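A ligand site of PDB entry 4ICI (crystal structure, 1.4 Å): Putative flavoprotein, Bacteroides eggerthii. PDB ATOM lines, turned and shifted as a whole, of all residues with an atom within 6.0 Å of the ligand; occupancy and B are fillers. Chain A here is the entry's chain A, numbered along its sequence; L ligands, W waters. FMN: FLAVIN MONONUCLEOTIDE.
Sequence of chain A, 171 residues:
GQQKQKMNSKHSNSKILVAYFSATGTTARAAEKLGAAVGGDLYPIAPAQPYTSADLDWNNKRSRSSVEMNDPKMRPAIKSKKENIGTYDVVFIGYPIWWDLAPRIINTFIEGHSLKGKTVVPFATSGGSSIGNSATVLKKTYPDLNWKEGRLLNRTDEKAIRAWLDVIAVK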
ATOM      1  N   PHE A  21     -10.077   6.995  -5.893  1.00  0.00           N
ATOM      2  CA  PHE A  21     -10.729   5.701  -5.777  1.00  0.00           C
ATOM      3  C   PHE A  21     -10.125   4.976  -4.568  1.00  0.00           C
ATOM      4  O   PHE A  21      -8.901   4.974  -4.364  1.00  0.00           O
ATOM      5  CB  PHE A  21     -10.488   4.891  -7.052  1.00  0.00           C
ATOM      6  CG  PHE A  21     -10.898   3.438  -6.962  1.00  0.00           C
ATOM      7  CD1 PHE A  21     -12.202   3.091  -6.694  1.00  0.00           C
ATOM      8  CD2 PHE A  21      -9.976   2.442  -7.144  1.00  0.00           C
ATOM      9  CE1 PHE A  21     -12.559   1.765  -6.592  1.00  0.00           C
ATOM     10  CE2 PHE A  21     -10.333   1.133  -7.055  1.00  0.00           C
ATOM     11  CZ  PHE A  21     -11.634   0.791  -6.766  1.00  0.00           C
ATOM     12  N   SER A  22     -10.996   4.369  -3.773  1.00  0.00           N
ATOM     13  CA  SER A  22     -10.575   3.568  -2.645  1.00  0.00           C
ATOM     14  C   SER A  22     -11.516   2.388  -2.514  1.00  0.00           C
ATOM     15  O   SER A  22     -12.740   2.564  -2.418  1.00  0.00           O
ATOM     16  CB  SER A  22     -10.615   4.403  -1.381  1.00  0.00           C
ATOM     17  OG  SER A  22     -10.104   3.678  -0.262  1.00  0.00           O
ATOM     18  N   ALA A  23     -10.961   1.191  -2.519  1.00  0.00           N
ATOM     19  CA  ALA A  23     -11.768  -0.024  -2.360  1.00  0.00           C
ATOM     20  C   ALA A  23     -11.929  -0.452  -0.917  1.00  0.00           C
ATOM     21  O   ALA A  23     -13.017  -0.955  -0.541  1.00  0.00           O
ATOM     22  CB  ALA A  23     -11.168  -1.168  -3.191  1.00  0.00           C
ATOM     23  N   THR A  24     -10.884  -0.291  -0.096  1.00  0.00           N
ATOM     24  CA  THR A  24     -10.959  -0.631   1.332  1.00  0.00           C
ATOM     25  C   THR A  24     -10.607   0.487   2.317  1.00  0.00           C
ATOM     26  O   THR A  24     -10.318   0.216   3.496  1.00  0.00           O
ATOM     27  CB  THR A  24     -10.124  -1.879   1.673  1.00  0.00           C
ATOM     28  OG1 THR A  24      -8.795  -1.788   1.169  1.00  0.00           O
ATOM     29  CG2 THR A  24     -10.813  -3.174   1.143  1.00  0.00           C
ATOM     30  N   GLY A  25     -10.655   1.735   1.853  1.00  0.00           N
ATOM     31  CA  GLY A  25     -10.557   2.871   2.761  1.00  0.00           C
ATOM     32  C   GLY A  25      -9.178   3.506   2.913  1.00  0.00           C
ATOM     33  O   GLY A  25      -9.070   4.614   3.403  1.00  0.00           O
ATOM     34  N   THR A  26      -8.113   2.774   2.551  1.00  0.00           N
ATOM     35  CA  THR A  26      -6.747   3.240   2.812  1.00  0.00           C
ATOM     36  C   THR A  26      -6.448   4.513   2.020  1.00  0.00           C
ATOM     37  O   THR A  26      -5.928   5.496   2.551  1.00  0.00           O
ATOM     38  CB  THR A  26      -5.698   2.172   2.473  1.00  0.00           C
ATOM     39  OG1 THR A  26      -6.091   0.908   3.021  1.00  0.00           O
ATOM     40  CG2 THR A  26      -4.312   2.542   2.989  1.00  0.00           C
ATOM     41  N   THR A  27      -6.783   4.485   0.742  1.00  0.00           N
ATOM     42  CA  THR A  27      -6.578   5.655  -0.114  1.00  0.00           C
ATOM     43  C   THR A  27      -7.523   6.786   0.260  1.00  0.00           C
ATOM     44  O   THR A  27      -7.152   7.957   0.149  1.00  0.00           O
ATOM     45  CB  THR A  27      -6.721   5.279  -1.600  1.00  0.00           C
ATOM     46  OG1 THR A  27      -5.927   4.115  -1.834  1.00  0.00           O
ATOM     47  CG2 THR A  27      -6.256   6.399  -2.507  1.00  0.00           C
ATOM     48  N   ALA A  28      -8.734   6.460   0.710  1.00  0.00           N
ATOM     49  CA  ALA A  28      -9.646   7.504   1.176  1.00  0.00           C
ATOM     50  C   ALA A  28      -9.015   8.298   2.340  1.00  0.00           C
ATOM     51  O   ALA A  28      -9.145   9.514   2.430  1.00  0.00           O
ATOM     52  CB  ALA A  28     -10.985   6.905   1.601  1.00  0.00           C
ATOM     53  N   ASP A  55     -13.990  -9.756  -5.285  1.00  0.00           N
ATOM     54  CA  ASP A  55     -13.519  -8.990  -6.425  1.00  0.00           C
ATOM     55  C   ASP A  55     -12.040  -8.631  -6.301  1.00  0.00           C
ATOM     56  O   ASP A  55     -11.339  -8.506  -7.304  1.00  0.00           O
ATOM     57  CB  ASP A  55     -14.294  -7.699  -6.599  1.00  0.00           C
ATOM     58  CG  ASP A  55     -15.736  -7.885  -7.093  1.00  0.00           C
ATOM     59  OD1 ASP A  55     -16.103  -8.947  -7.625  1.00  0.00           O
ATOM     60  OD2 ASP A  55     -16.453  -6.863  -7.007  1.00  0.00           O
ATOM     61  N   LEU A  56     -11.622  -8.365  -5.058  1.00  0.00           N
ATOM     62  CA  LEU A  56     -10.263  -7.905  -4.747  1.00  0.00           C
ATOM     63  C   LEU A  56      -9.239  -9.028  -4.501  1.00  0.00           C
ATOM     64  O   LEU A  56      -8.116  -8.762  -4.100  1.00  0.00           O
ATOM     65  CB  LEU A  56     -10.333  -6.977  -3.539  1.00  0.00           C
ATOM     66  CG  LEU A  56     -11.210  -5.727  -3.727  1.00  0.00           C
ATOM     67  CD1 LEU A  56     -11.467  -4.970  -2.375  1.00  0.00           C
ATOM     68  CD2 LEU A  56     -10.669  -4.788  -4.817  1.00  0.00           C
ATOM     69  N   ASP A  57      -9.631 -10.268  -4.775  1.00  0.00           N
ATOM     70  CA  ASP A  57      -8.756 -11.410  -4.508  1.00  0.00           C
ATOM     71  C   ASP A  57      -7.733 -11.530  -5.633  1.00  0.00           C
ATOM     72  O   ASP A  57      -7.987 -12.110  -6.689  1.00  0.00           O
ATOM     73  CB  ASP A  57      -9.562 -12.694  -4.350  1.00  0.00           C
ATOM     74  CG  ASP A  57      -8.700 -13.879  -3.907  1.00  0.00           C
ATOM     75  OD1 ASP A  57      -7.462 -13.711  -3.827  1.00  0.00           O
ATOM     76  OD2 ASP A  57      -9.270 -14.978  -3.671  1.00  0.00           O
ATOM     77  N   TRP A  58      -6.531 -11.002  -5.365  1.00  0.00           N
ATOM     78  CA  TRP A  58      -5.431 -11.072  -6.337  1.00  0.00           C
ATOM     79  C   TRP A  58      -4.833 -12.463  -6.527  1.00  0.00           C
ATOM     80  O   TRP A  58      -4.042 -12.657  -7.439  1.00  0.00           O
ATOM     81  CB  TRP A  58      -4.323 -10.060  -5.974  1.00  0.00           C
ATOM     82  CG  TRP A  58      -3.684 -10.348  -4.686  1.00  0.00           C
ATOM     83  CD1 TRP A  58      -2.801 -11.375  -4.402  1.00  0.00           C
ATOM     84  CD2 TRP A  58      -3.852  -9.629  -3.472  1.00  0.00           C
ATOM     85  NE1 TRP A  58      -2.431 -11.330  -3.087  1.00  0.00           N
ATOM     86  CE2 TRP A  58      -3.048 -10.257  -2.492  1.00  0.00           C
ATOM     87  CE3 TRP A  58      -4.579  -8.502  -3.122  1.00  0.00           C
ATOM     88  CZ2 TRP A  58      -2.974  -9.798  -1.185  1.00  0.00           C
ATOM     89  CZ3 TRP A  58      -4.513  -8.037  -1.816  1.00  0.00           C
ATOM     90  CH2 TRP A  58      -3.704  -8.676  -0.857  1.00  0.00           C
ATOM     91  N   SER A  65     -10.973  -8.025 -10.210  1.00  0.00           N
ATOM     92  CA  SER A  65      -9.775  -7.191 -10.298  1.00  0.00           C
ATOM     93  C   SER A  65      -8.708  -7.828 -11.196  1.00  0.00           C
ATOM     94  O   SER A  65      -8.056  -7.113 -11.951  1.00  0.00           O
ATOM     95  CB  SER A  65      -9.206  -6.857  -8.911  1.00  0.00           C
ATOM     96  OG  SER A  65      -8.772  -7.992  -8.171  1.00  0.00           O
ATOM     97  N   SER A  66      -8.584  -9.150 -11.175  1.00  0.00           N
ATOM     98  CA  SER A  66      -7.607  -9.794 -12.064  1.00  0.00           C
ATOM     99  C   SER A  66      -7.983  -9.612 -13.524  1.00  0.00           C
ATOM    100  O   SER A  66      -7.129  -9.327 -14.362  1.00  0.00           O
ATOM    101  CB  SER A  66      -7.500 -11.282 -11.757  1.00  0.00           C
ATOM    102  OG  SER A  66      -6.901 -11.472 -10.497  1.00  0.00           O
ATOM    103  N   MET A  69      -7.298  -6.039 -14.600  1.00  0.00           N
ATOM    104  CA  MET A  69      -5.922  -5.687 -14.758  1.00  0.00           C
ATOM    105  C   MET A  69      -5.343  -6.362 -16.022  1.00  0.00           C
ATOM    106  O   MET A  69      -4.435  -5.816 -16.653  1.00  0.00           O
ATOM    107  CB  MET A  69      -5.195  -5.917 -13.436  1.00  0.00           C
ATOM    108  CG  MET A  69      -5.690  -4.934 -12.263  1.00  0.00           C
ATOM    109  SD  MET A  69      -6.178  -3.089 -12.669  1.00  0.00           S
ATOM    110  CE  MET A  69      -4.519  -2.372 -13.196  1.00  0.00           C
ATOM    111  N   TYR A  95      -5.334   6.602  -5.856  1.00  0.00           N
ATOM    112  CA  TYR A  95      -5.716   5.206  -6.082  1.00  0.00           C
ATOM    113  C   TYR A  95      -4.862   4.274  -5.247  1.00  0.00           C
ATOM    114  O   TYR A  95      -3.715   4.571  -4.936  1.00  0.00           O
ATOM    115  CB  TYR A  95      -5.625   4.832  -7.578  1.00  0.00           C
ATOM    116  CG  TYR A  95      -4.326   5.255  -8.255  1.00  0.00           C
ATOM    117  CD1 TYR A  95      -4.197   6.506  -8.824  1.00  0.00           C
ATOM    118  CD2 TYR A  95      -3.253   4.413  -8.292  1.00  0.00           C
ATOM    119  CE1 TYR A  95      -2.984   6.898  -9.407  1.00  0.00           C
ATOM    120  CE2 TYR A  95      -2.052   4.788  -8.870  1.00  0.00           C
ATOM    121  CZ  TYR A  95      -1.924   6.021  -9.424  1.00  0.00           C
ATOM    122  OH  TYR A  95      -0.728   6.442  -9.994  1.00  0.00           O
ATOM    123  N   PRO A  96      -5.372   3.072  -4.987  1.00  0.00           N
ATOM    124  CA  PRO A  96      -4.530   1.978  -4.537  1.00  0.00           C
ATOM    125  C   PRO A  96      -3.728   1.436  -5.716  1.00  0.00           C
ATOM    126  O   PRO A  96      -4.234   1.416  -6.847  1.00  0.00           O
ATOM    127  CB  PRO A  96      -5.534   0.937  -4.074  1.00  0.00           C
ATOM    128  CG  PRO A  96      -6.741   1.151  -4.953  1.00  0.00           C
ATOM    129  CD  PRO A  96      -6.774   2.644  -5.179  1.00  0.00           C
ATOM    130  N   ILE A  97      -2.510   1.007  -5.491  1.00  0.00           N
ATOM    131  CA  ILE A  97      -1.706   0.318  -6.516  1.00  0.00           C
ATOM    132  C   ILE A  97      -2.246  -1.092  -6.694  1.00  0.00           C
ATOM    133  O   ILE A  97      -2.311  -1.829  -5.725  1.00  0.00           O
ATOM    134  CB  ILE A  97      -0.217   0.200  -6.124  1.00  0.00           C
ATOM    135  CG1 ILE A  97       0.445   1.575  -5.941  1.00  0.00           C
ATOM    136  CG2 ILE A  97       0.567  -0.674  -7.146  1.00  0.00           C
ATOM    137  CD1 ILE A  97       0.313   2.523  -7.150  1.00  0.00           C
ATOM    138  N   TRP A  98      -2.665  -1.462  -7.897  1.00  0.00           N
ATOM    139  CA  TRP A  98      -3.102  -2.805  -8.245  1.00  0.00           C
ATOM    140  C   TRP A  98      -2.200  -3.342  -9.355  1.00  0.00           C
ATOM    141  O   TRP A  98      -2.164  -2.793 -10.449  1.00  0.00           O
ATOM    142  CB  TRP A  98      -4.548  -2.823  -8.730  1.00  0.00           C
ATOM    143  CG  TRP A  98      -5.599  -2.661  -7.704  1.00  0.00           C
ATOM    144  CD1 TRP A  98      -5.452  -2.375  -6.368  1.00  0.00           C
ATOM    145  CD2 TRP A  98      -7.014  -2.672  -7.939  1.00  0.00           C
ATOM    146  NE1 TRP A  98      -6.685  -2.254  -5.763  1.00  0.00           N
ATOM    147  CE2 TRP A  98      -7.650  -2.430  -6.707  1.00  0.00           C
ATOM    148  CE3 TRP A  98      -7.805  -2.890  -9.073  1.00  0.00           C
ATOM    149  CZ2 TRP A  98      -9.039  -2.400  -6.565  1.00  0.00           C
ATOM    150  CZ3 TRP A  98      -9.178  -2.855  -8.916  1.00  0.00           C
ATOM    151  CH2 TRP A  98      -9.775  -2.607  -7.668  1.00  0.00           C
ATOM    152  N   TRP A  99      -1.438  -4.399  -9.043  1.00  0.00           N
ATOM    153  CA  TRP A  99      -0.495  -4.972  -9.996  1.00  0.00           C
ATOM    154  C   TRP A  99       0.418  -3.894 -10.619  1.00  0.00           C
ATOM    155  O   TRP A  99       0.676  -3.874 -11.823  1.00  0.00           O
ATOM    156  CB  TRP A  99      -1.266  -5.751 -11.060  1.00  0.00           C
ATOM    157  CG  TRP A  99      -2.024  -6.908 -10.508  1.00  0.00           C
ATOM    158  CD1 TRP A  99      -3.351  -6.951 -10.123  1.00  0.00           C
ATOM    159  CD2 TRP A  99      -1.485  -8.215 -10.190  1.00  0.00           C
ATOM    160  NE1 TRP A  99      -3.648  -8.185  -9.620  1.00  0.00           N
ATOM    161  CE2 TRP A  99      -2.539  -8.975  -9.647  1.00  0.00           C
ATOM    162  CE3 TRP A  99      -0.224  -8.794 -10.334  1.00  0.00           C
ATOM    163  CZ2 TRP A  99      -2.357 -10.297  -9.234  1.00  0.00           C
ATOM    164  CZ3 TRP A  99      -0.046 -10.122  -9.914  1.00  0.00           C
ATOM    165  CH2 TRP A  99      -1.116 -10.853  -9.371  1.00  0.00           C
ATOM    166  N   ASP A 100       0.926  -3.016  -9.757  1.00  0.00           N
ATOM    167  CA  ASP A 100       1.854  -1.936 -10.132  1.00  0.00           C
ATOM    168  C   ASP A 100       1.251  -0.897 -11.080  1.00  0.00           C
ATOM    169  O   ASP A 100       1.988  -0.160 -11.746  1.00  0.00           O
ATOM    170  CB  ASP A 100       3.171  -2.513 -10.711  1.00  0.00           C
ATOM    171  CG  ASP A 100       4.415  -1.709 -10.338  1.00  0.00           C
ATOM    172  OD1 ASP A 100       4.346  -0.764  -9.497  1.00  0.00           O
ATOM    173  OD2 ASP A 100       5.453  -2.039 -10.956  1.00  0.00           O
ATOM    174  N   LEU A 101      -0.080  -0.829 -11.119  1.00  0.00           N
ATOM    175  CA  LEU A 101      -0.801   0.081 -11.990  1.00  0.00           C
ATOM    176  C   LEU A 101      -1.918   0.813 -11.235  1.00  0.00           C
ATOM    177  O   LEU A 101      -2.311   0.418 -10.150  1.00  0.00           O
ATOM    178  CB  LEU A 101      -1.448  -0.702 -13.155  1.00  0.00           C
ATOM    179  CG  LEU A 101      -0.507  -1.367 -14.158  1.00  0.00           C
ATOM    180  CD1 LEU A 101      -1.321  -2.387 -15.002  1.00  0.00           C
ATOM    181  CD2 LEU A 101       0.214  -0.315 -15.018  1.00  0.00           C
ATOM    182  N   THR A 125      -1.796   4.734  -2.421  1.00  0.00           N
ATOM    183  CA  THR A 125      -1.394   3.870  -1.317  1.00  0.00           C
ATOM    184  C   THR A 125      -1.105   2.489  -1.862  1.00  0.00           C
ATOM    185  O   THR A 125      -1.525   2.140  -2.959  1.00  0.00           O
ATOM    186  CB  THR A 125      -2.441   3.816  -0.167  1.00  0.00           C
ATOM    187  OG1 THR A 125      -3.611   3.117  -0.563  1.00  0.00           O
ATOM    188  CG2 THR A 125      -2.794   5.209   0.362  1.00  0.00           C
ATOM    189  N   SER A 126      -0.337   1.690  -1.114  1.00  0.00           N
ATOM    190  CA  SER A 126       0.098   0.367  -1.587  1.00  0.00           C
ATOM    191  C   SER A 126       0.530  -0.486  -0.425  1.00  0.00           C
ATOM    192  O   SER A 126       0.702  -0.001   0.718  1.00  0.00           O
ATOM    193  CB  SER A 126       1.267   0.482  -2.546  1.00  0.00           C
ATOM    194  OG  SER A 126       2.477   0.749  -1.850  1.00  0.00           O
ATOM    195  N   GLY A 127       0.755  -1.738  -0.767  1.00  0.00           N
ATOM    196  CA  GLY A 127       1.363  -2.702   0.148  1.00  0.00           C
ATOM    197  C   GLY A 127       2.878  -2.721   0.112  1.00  0.00           C
ATOM    198  O   GLY A 127       3.480  -3.661   0.658  1.00  0.00           O
ATOM    199  N   GLY A 128       3.484  -1.714  -0.507  1.00  0.00           N
ATOM    200  CA  GLY A 128       4.947  -1.673  -0.658  1.00  0.00           C
ATOM    201  C   GLY A 128       5.437  -1.118  -1.984  1.00  0.00           C
ATOM    202  O   GLY A 128       6.528  -0.504  -2.053  1.00  0.00           O
ATOM    203  N   SER A 129       4.700  -1.377  -3.060  1.00  0.00           N
ATOM    204  CA  SER A 129       5.131  -0.886  -4.347  1.00  0.00           C
ATOM    205  C   SER A 129       5.204   0.633  -4.347  1.00  0.00           C
ATOM    206  O   SER A 129       4.372   1.311  -3.734  1.00  0.00           O
ATOM    207  CB  SER A 129       4.171  -1.308  -5.443  1.00  0.00           C
ATOM    208  OG  SER A 129       4.257  -2.701  -5.702  1.00  0.00           O
ATOM    209  N   SER A 130       6.160   1.153  -5.104  1.00  0.00           N
ATOM    210  CA  SER A 130       6.274   2.578  -5.338  1.00  0.00           C
ATOM    211  C   SER A 130       5.203   3.014  -6.334  1.00  0.00           C
ATOM    212  O   SER A 130       4.640   2.203  -7.084  1.00  0.00           O
ATOM    213  CB  SER A 130       7.641   2.930  -5.886  1.00  0.00           C
ATOM    214  OG  SER A 130       7.847   2.316  -7.131  1.00  0.00           O
ATOM    215  N   ASN A 154       1.380   6.273   1.908  1.00  0.00           N
ATOM    216  CA  ASN A 154       1.109   5.262   2.933  1.00  0.00           C
ATOM    217  C   ASN A 154       1.255   5.812   4.337  1.00  0.00           C
ATOM    218  O   ASN A 154       0.471   5.476   5.234  1.00  0.00           O
ATOM    219  CB  ASN A 154       2.035   4.046   2.769  1.00  0.00           C
ATOM    220  CG  ASN A 154       1.672   3.197   1.569  1.00  0.00           C
ATOM    221  OD1 ASN A 154       0.516   3.196   1.156  1.00  0.00           O
ATOM    222  ND2 ASN A 154       2.641   2.472   1.005  1.00  0.00           N
HETATM  223  N1  FMN L   1       0.216  -3.417  -3.250  1.00  0.00           N
HETATM  224  C2  FMN L   1       1.472  -3.257  -3.771  1.00  0.00           C
HETATM  225  O2  FMN L   1       2.361  -2.801  -3.046  1.00  0.00           O
HETATM  226  N3  FMN L   1       1.729  -3.610  -5.081  1.00  0.00           N
HETATM  227  C4  FMN L   1       0.773  -4.169  -5.910  1.00  0.00           C
HETATM  228  O4  FMN L   1       1.108  -4.402  -7.094  1.00  0.00           O
HETATM  229  C4A FMN L   1      -0.513  -4.370  -5.370  1.00  0.00           C
HETATM  230  N5  FMN L   1      -1.524  -4.970  -6.153  1.00  0.00           N
HETATM  231  C5A FMN L   1      -2.800  -5.103  -5.576  1.00  0.00           C
HETATM  232  C6  FMN L   1      -3.829  -5.657  -6.345  1.00  0.00           C
HETATM  233  C7  FMN L   1      -5.090  -5.789  -5.817  1.00  0.00           C
HETATM  234  C7M FMN L   1      -6.205  -6.331  -6.661  1.00  0.00           C
HETATM  235  C8  FMN L   1      -5.366  -5.378  -4.528  1.00  0.00           C
HETATM  236  C8M FMN L   1      -6.752  -5.546  -3.950  1.00  0.00           C
HETATM  237  C9  FMN L   1      -4.345  -4.835  -3.760  1.00  0.00           C
HETATM  238  C9A FMN L   1      -3.048  -4.669  -4.279  1.00  0.00           C
HETATM  239  N10 FMN L   1      -2.007  -4.114  -3.516  1.00  0.00           N
HETATM  240  C10 FMN L   1      -0.758  -3.965  -4.052  1.00  0.00           C
HETATM  241  C1' FMN L   1      -2.290  -3.618  -2.113  1.00  0.00           C
HETATM  242  C2' FMN L   1      -2.983  -2.224  -2.218  1.00  0.00           C
HETATM  243  O2' FMN L   1      -2.308  -1.305  -3.047  1.00  0.00           O
HETATM  244  C3' FMN L   1      -3.052  -1.530  -0.844  1.00  0.00           C
HETATM  245  O3' FMN L   1      -3.561  -2.461   0.171  1.00  0.00           O
HETATM  246  C4' FMN L   1      -3.848  -0.189  -0.855  1.00  0.00           C
HETATM  247  O4' FMN L   1      -3.481   0.523   0.301  1.00  0.00           O
HETATM  248  C5' FMN L   1      -5.400  -0.483  -0.776  1.00  0.00           C
HETATM  249  O5' FMN L   1      -6.014   0.784  -0.808  1.00  0.00           O
HETATM  250  P   FMN L   1      -7.581   0.984  -0.559  1.00  0.00           P
HETATM  251  O1P FMN L   1      -7.808   0.533   0.895  1.00  0.00           O
HETATM  252  O2P FMN L   1      -7.917   2.373  -0.851  1.00  0.00           O
HETATM  253  O3P FMN L   1      -8.390   0.105  -1.514  1.00  0.00           O
HETATM  254  O   HOH W   1      -1.636   0.168   2.301  1.00  0.00           O
HETATM  255  O   HOH W   2      -1.593  -3.785   1.404  1.00  0.00           O
HETATM  256  O   HOH W   3       3.326  -5.398  -8.236  1.00  0.00           O
HETATM  257  O   HOH W   4      -4.531  -1.390   2.900  1.00  0.00           O
HETATM  258  O   HOH W   5      -7.546  -1.968  -3.012  1.00  0.00           O
HETATM  259  O   HOH W   6      -5.469  -4.399  -0.354  1.00  0.00           O
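Water W5 bridges O3P of the ligand (2.7 Å) and NE1 of Trp 98 (2.9 Å).
Water W1 lies within hydrogen-bond range of an oxygen (O4') of the ligand (2.7 Å) and the backbone carbonyl oxygen of Ser 126 (2.8 Å).
Water W4 lies within hydrogen-bond range of OG1 of Thr 26 and O3' of the ligand.
Residues that only touch the ligand: Leu 56 (3.5 Å), Trp 58 (3.5 Å), Ser 65 (3.4 Å), Pro 96 (3.3 Å), Trp 98 (3.4 Å) and Ser 126 (3.3 Å).
Of the 29 residues printed, 19 come within 4 Å of the ligand.
Along chain A the residues within 4 Å of the ligand span positions 22 to 129.
The nearest printed residue that does not touch the ligand is Ala 28 (4.5 Å).
An oxygen (O3P) of the ligand is in hydrogen-bond range of the backbone NH (N) of Thr 24 (2.9 Å).
The side-chain hydroxyl (OG1) of Thr 24 lies within hydrogen-bond range of an oxygen (O1P) of the ligand (2.5 Å).
An oxygen (O2P) of the ligand sits at hydrogen-bond distance from the side-chain hydroxyl (OG) of Ser 22 (2.6 Å).
N of Ile 97 is in hydrogen-bond range of O2' of the ligand.
O2' of the ligand is in hydrogen-bond range of O of Ile 97 (2.7 Å).
The side-chain hydroxyl (OG1) of Thr 125 lies within hydrogen-bond range of an oxygen (O4') of the ligand (2.7 Å).
N of Ser 129 is in hydrogen-bond range of O2 of the ligand (2.7 Å).
The side-chain hydroxyl of Ser 129 is in hydrogen-bond range of a nitrogen (N3) of the ligand.
N of Thr 26 is in hydrogen-bond range of O1P of the ligand, 2.8 Å away.
OG1 of Thr 26 sits at hydrogen-bond distance from O1P of the ligand (2.8 Å).
N of Thr 27 sits at hydrogen-bond distance from O2P of the ligand, 2.9 Å away.
An oxygen (O2P) of the ligand lies within hydrogen-bond range of the side-chain hydroxyl (OG1) of Thr 27, 2.8 Å away.
The backbone NH (N) of Trp 99 lies within hydrogen-bond range of a nitrogen (N5) of the ligand (2.9 Å).
The backbone NH of Ala 23 sits at hydrogen-bond distance from an oxygen (O3P) of the ligand, at 3.0 Å.
The backbone NH (N) of Gly 128 is in hydrogen-bond range of an oxygen (O2) of the ligand (3.0 Å).
An oxygen (O2) of the ligand is in hydrogen-bond range of the backbone NH of Gly 127.
The backbone NH (N) of Asp 100 is in hydrogen-bond range of an oxygen (O4) of the ligand (3.0 Å).
The backbone NH of Gly 25 is in hydrogen-bond range of an oxygen (O1P) of the ligand (3.2 Å).
N of Gly 25 lies within hydrogen-bond range of OG of Ser 22, at 2.9 Å.
The backbone NH of Ile 97 lies within hydrogen-bond range of the backbone carbonyl oxygen of Thr 125 (2.9 Å).
OG1 of Thr 125 lies within hydrogen-bond range of OG1 of Thr 27.
The backbone carbonyl oxygen of Tyr 95 sits at hydrogen-bond distance from the backbone NH of Thr 125.
OG of Ser 126 lies within hydrogen-bond range of O of Ser 129 (2.7 Å).
N of Gly 128 lies within hydrogen-bond range of OG of Ser 126 (3.0 Å).
The side-chain amide oxygen (OD1) of Asn 154 sits at hydrogen-bond distance from the backbone NH (N) of Ser 126.
The side-chain hydroxyl (OG) of Ser 65 sits at hydrogen-bond distance from the backbone carbonyl oxygen (O) of Asp 55 (2.8 Å).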
